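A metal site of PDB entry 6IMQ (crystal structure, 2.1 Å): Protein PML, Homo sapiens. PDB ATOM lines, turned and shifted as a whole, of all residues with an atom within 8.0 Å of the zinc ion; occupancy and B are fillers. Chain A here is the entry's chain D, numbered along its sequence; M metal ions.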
ATOM      1  N   VAL A  11     -23.627 -34.011   8.103  1.00  0.00           N
ATOM      2  CA  VAL A  11     -24.106 -33.048   7.119  1.00  0.00           C
ATOM      3  C   VAL A  11     -23.063 -31.957   6.904  1.00  0.00           C
ATOM      4  O   VAL A  11     -22.309 -31.581   7.826  1.00  0.00           O
ATOM      5  CB  VAL A  11     -25.464 -32.406   7.490  1.00  0.00           C
ATOM      6  CG1 VAL A  11     -26.538 -33.466   7.653  1.00  0.00           C
ATOM      7  CG2 VAL A  11     -25.335 -31.547   8.744  1.00  0.00           C
ATOM      8  N   CYS A  12     -23.022 -31.442   5.677  1.00  0.00           N
ATOM      9  CA  CYS A  12     -22.283 -30.217   5.365  1.00  0.00           C
ATOM     10  C   CYS A  12     -22.659 -29.098   6.322  1.00  0.00           C
ATOM     11  O   CYS A  12     -23.826 -28.958   6.717  1.00  0.00           O
ATOM     12  CB  CYS A  12     -22.592 -29.821   3.921  1.00  0.00           C
ATOM     13  SG  CYS A  12     -21.902 -28.286   3.325  1.00  0.00           S
ATOM     14  N   THR A  13     -21.663 -28.303   6.714  1.00  0.00           N
ATOM     15  CA  THR A  13     -21.919 -27.260   7.679  1.00  0.00           C
ATOM     16  C   THR A  13     -22.648 -26.065   7.077  1.00  0.00           C
ATOM     17  O   THR A  13     -23.169 -25.234   7.817  1.00  0.00           O
ATOM     18  CB  THR A  13     -20.623 -26.740   8.307  1.00  0.00           C
ATOM     19  OG1 THR A  13     -19.941 -25.907   7.353  1.00  0.00           O
ATOM     20  CG2 THR A  13     -19.709 -27.873   8.711  1.00  0.00           C
ATOM     21  N   ARG A  14     -22.646 -25.927   5.748  1.00  0.00           N
ATOM     22  CA  ARG A  14     -23.273 -24.791   5.088  1.00  0.00           C
ATOM     23  C   ARG A  14     -24.655 -25.101   4.545  1.00  0.00           C
ATOM     24  O   ARG A  14     -25.531 -24.230   4.553  1.00  0.00           O
ATOM     25  CB  ARG A  14     -22.383 -24.293   3.949  1.00  0.00           C
ATOM     26  CG  ARG A  14     -23.014 -23.226   3.062  1.00  0.00           C
ATOM     27  CD  ARG A  14     -22.001 -22.555   2.108  1.00  0.00           C
ATOM     28  NE  ARG A  14     -22.680 -21.621   1.221  1.00  0.00           N
ATOM     29  CZ  ARG A  14     -22.794 -21.765  -0.103  1.00  0.00           C
ATOM     30  NH1 ARG A  14     -22.253 -22.806  -0.714  1.00  0.00           N
ATOM     31  NH2 ARG A  14     -23.463 -20.855  -0.802  1.00  0.00           N
ATOM     32  N   CYS A  15     -24.864 -26.323   4.062  1.00  0.00           N
ATOM     33  CA  CYS A  15     -26.157 -26.781   3.571  1.00  0.00           C
ATOM     34  C   CYS A  15     -26.791 -27.680   4.631  1.00  0.00           C
ATOM     35  O   CYS A  15     -26.486 -27.572   5.820  1.00  0.00           O
ATOM     36  CB  CYS A  15     -25.958 -27.497   2.236  1.00  0.00           C
ATOM     37  SG  CYS A  15     -25.617 -26.397   0.845  1.00  0.00           S
ATOM     38  N   LYS A  16     -27.685 -28.572   4.217  1.00  0.00           N
ATOM     39  CA  LYS A  16     -28.111 -29.688   5.031  1.00  0.00           C
ATOM     40  C   LYS A  16     -27.796 -31.014   4.354  1.00  0.00           C
ATOM     41  O   LYS A  16     -28.237 -32.069   4.819  1.00  0.00           O
ATOM     42  CB  LYS A  16     -29.612 -29.590   5.353  1.00  0.00           C
ATOM     43  CG  LYS A  16     -29.872 -28.965   6.726  1.00  0.00           C
ATOM     44  CD  LYS A  16     -31.266 -28.375   6.829  1.00  0.00           C
ATOM     45  CE  LYS A  16     -31.962 -28.847   8.105  1.00  0.00           C
ATOM     46  NZ  LYS A  16     -33.262 -28.151   8.346  1.00  0.00           N
ATOM     47  N   GLU A  17     -26.992 -30.980   3.285  1.00  0.00           N
ATOM     48  CA  GLU A  17     -26.771 -32.135   2.428  1.00  0.00           C
ATOM     49  C   GLU A  17     -25.727 -33.086   3.010  1.00  0.00           C
ATOM     50  O   GLU A  17     -25.433 -33.050   4.207  1.00  0.00           O
ATOM     51  CB  GLU A  17     -26.338 -31.680   1.037  1.00  0.00           C
ATOM     52  CG  GLU A  17     -27.142 -32.263  -0.097  1.00  0.00           C
ATOM     53  CD  GLU A  17     -26.327 -32.438  -1.358  1.00  0.00           C
ATOM     54  OE1 GLU A  17     -25.356 -31.680  -1.556  1.00  0.00           O
ATOM     55  OE2 GLU A  17     -26.640 -33.360  -2.143  1.00  0.00           O
ATOM     56  N   SER A  18     -25.175 -33.940   2.150  1.00  0.00           N
ATOM     57  CA  SER A  18     -24.315 -35.035   2.571  1.00  0.00           C
ATOM     58  C   SER A  18     -22.870 -34.596   2.634  1.00  0.00           C
ATOM     59  O   SER A  18     -22.272 -34.249   1.616  1.00  0.00           O
ATOM     60  CB  SER A  18     -24.467 -36.210   1.596  1.00  0.00           C
ATOM     61  OG  SER A  18     -24.101 -35.849   0.274  1.00  0.00           O
ATOM     62  N   ALA A  19     -22.298 -34.608   3.843  1.00  0.00           N
ATOM     63  CA  ALA A  19     -20.898 -34.264   3.999  1.00  0.00           C
ATOM     64  C   ALA A  19     -20.058 -35.202   3.147  1.00  0.00           C
ATOM     65  O   ALA A  19     -20.122 -36.427   3.296  1.00  0.00           O
ATOM     66  CB  ALA A  19     -20.480 -34.360   5.469  1.00  0.00           C
ATOM     67  N   ASP A  20     -19.309 -34.620   2.202  1.00  0.00           N
ATOM     68  CA  ASP A  20     -18.435 -35.394   1.330  1.00  0.00           C
ATOM     69  C   ASP A  20     -16.963 -35.143   1.571  1.00  0.00           C
ATOM     70  O   ASP A  20     -16.126 -35.942   1.133  1.00  0.00           O
ATOM     71  CB  ASP A  20     -18.740 -35.080  -0.143  1.00  0.00           C
ATOM     72  CG  ASP A  20     -19.376 -36.250  -0.877  1.00  0.00           C
ATOM     73  OD1 ASP A  20     -19.965 -37.132  -0.223  1.00  0.00           O
ATOM     74  OD2 ASP A  20     -19.277 -36.289  -2.125  1.00  0.00           O
ATOM     75  N   LEU A  29     -16.916 -29.737   7.870  1.00  0.00           N
ATOM     76  CA  LEU A  29     -17.420 -30.714   6.918  1.00  0.00           C
ATOM     77  C   LEU A  29     -18.169 -30.017   5.786  1.00  0.00           C
ATOM     78  O   LEU A  29     -18.915 -29.059   6.031  1.00  0.00           O
ATOM     79  CB  LEU A  29     -18.340 -31.710   7.614  1.00  0.00           C
ATOM     80  CG  LEU A  29     -17.713 -32.723   8.576  1.00  0.00           C
ATOM     81  CD1 LEU A  29     -18.743 -33.175   9.606  1.00  0.00           C
ATOM     82  CD2 LEU A  29     -17.172 -33.897   7.788  1.00  0.00           C
ATOM     83  N   LEU A  30     -17.994 -30.507   4.568  1.00  0.00           N
ATOM     84  CA  LEU A  30     -18.560 -29.868   3.389  1.00  0.00           C
ATOM     85  C   LEU A  30     -19.112 -30.900   2.413  1.00  0.00           C
ATOM     86  O   LEU A  30     -18.586 -32.004   2.294  1.00  0.00           O
ATOM     87  CB  LEU A  30     -17.515 -29.000   2.673  1.00  0.00           C
ATOM     88  CG  LEU A  30     -17.034 -27.783   3.458  1.00  0.00           C
ATOM     89  CD1 LEU A  30     -15.914 -27.093   2.684  1.00  0.00           C
ATOM     90  CD2 LEU A  30     -18.179 -26.828   3.740  1.00  0.00           C
ATOM     91  N   CYS A  31     -20.182 -30.511   1.709  1.00  0.00           N
ATOM     92  CA  CYS A  31     -20.675 -31.327   0.600  1.00  0.00           C
ATOM     93  C   CYS A  31     -19.787 -31.127  -0.622  1.00  0.00           C
ATOM     94  O   CYS A  31     -18.942 -30.228  -0.676  1.00  0.00           O
ATOM     95  CB  CYS A  31     -22.131 -30.990   0.271  1.00  0.00           C
ATOM     96  SG  CYS A  31     -22.421 -29.395  -0.519  1.00  0.00           S
ATOM     97  N   ALA A  32     -19.998 -31.975  -1.627  1.00  0.00           N
ATOM     98  CA  ALA A  32     -19.187 -31.909  -2.840  1.00  0.00           C
ATOM     99  C   ALA A  32     -19.280 -30.544  -3.507  1.00  0.00           C
ATOM    100  O   ALA A  32     -18.279 -30.009  -3.988  1.00  0.00           O
ATOM    101  CB  ALA A  32     -19.627 -33.001  -3.823  1.00  0.00           C
ATOM    102  N   LYS A  33     -20.492 -29.964  -3.545  1.00  0.00           N
ATOM    103  CA  LYS A  33     -20.687 -28.698  -4.240  1.00  0.00           C
ATOM    104  C   LYS A  33     -20.083 -27.536  -3.455  1.00  0.00           C
ATOM    105  O   LYS A  33     -19.280 -26.758  -4.003  1.00  0.00           O
ATOM    106  CB  LYS A  33     -22.189 -28.478  -4.466  1.00  0.00           C
ATOM    107  CG  LYS A  33     -22.565 -27.828  -5.805  1.00  0.00           C
ATOM    108  CD  LYS A  33     -22.035 -28.598  -7.008  1.00  0.00           C
ATOM    109  CE  LYS A  33     -22.507 -27.980  -8.330  1.00  0.00           C
ATOM    110  NZ  LYS A  33     -22.148 -26.541  -8.464  1.00  0.00           N
ATOM    111  N   CYS A  34     -20.424 -27.404  -2.179  1.00  0.00           N
ATOM    112  CA  CYS A  34     -19.809 -26.383  -1.351  1.00  0.00           C
ATOM    113  C   CYS A  34     -18.291 -26.549  -1.288  1.00  0.00           C
ATOM    114  O   CYS A  34     -17.572 -25.549  -1.230  1.00  0.00           O
ATOM    115  CB  CYS A  34     -20.405 -26.417   0.055  1.00  0.00           C
ATOM    116  SG  CYS A  34     -22.178 -26.087   0.079  1.00  0.00           S
ATOM    117  N   PHE A  35     -17.802 -27.794  -1.320  1.00  0.00           N
ATOM    118  CA  PHE A  35     -16.355 -27.972  -1.295  1.00  0.00           C
ATOM    119  C   PHE A  35     -15.720 -27.405  -2.560  1.00  0.00           C
ATOM    120  O   PHE A  35     -14.646 -26.792  -2.483  1.00  0.00           O
ATOM    121  CB  PHE A  35     -16.004 -29.443  -1.144  1.00  0.00           C
ATOM    122  CG  PHE A  35     -14.525 -29.693  -1.145  1.00  0.00           C
ATOM    123  CD1 PHE A  35     -13.756 -29.327  -0.057  1.00  0.00           C
ATOM    124  CD2 PHE A  35     -13.917 -30.284  -2.232  1.00  0.00           C
ATOM    125  CE1 PHE A  35     -12.395 -29.557  -0.053  1.00  0.00           C
ATOM    126  CE2 PHE A  35     -12.559 -30.524  -2.229  1.00  0.00           C
ATOM    127  CZ  PHE A  35     -11.810 -30.163  -1.129  1.00  0.00           C
HETATM  128 ZN    ZN M   1     -23.048 -28.040   1.204  1.00  0.00          ZN
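SG of Cys 15 touches the zinc ion, 3.1 Å away.
Of the 17 residues printed, 4 come within 4 Å of the zinc ion.
N of Lys 33 lies close to SG of Cys 31, at 3.6 Å.
N of Cys 15 lies close to SG of Cys 12, at 3.6 Å.
SG of Cys 34 lies close to NH1 of Arg 14 (3.4 Å).
The backbone NH (N) of Cys 12 sits at hydrogen-bond distance from the backbone carbonyl oxygen (O) of Glu 17 (3.2 Å).
The side-chain sulfur of Cys 34 sits close to the side-chain sulfur of Cys 15, 3.5 Å away.
SG of Cys 12 lies close to N of Arg 14 (3.5 Å).
The zinc ion is bound by the side-chain sulfur of Cys 31 (2.3 Å), the side-chain sulfur of Cys 34 (2.4 Å) and the side-chain sulfur of Cys 12 (2.4 Å).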
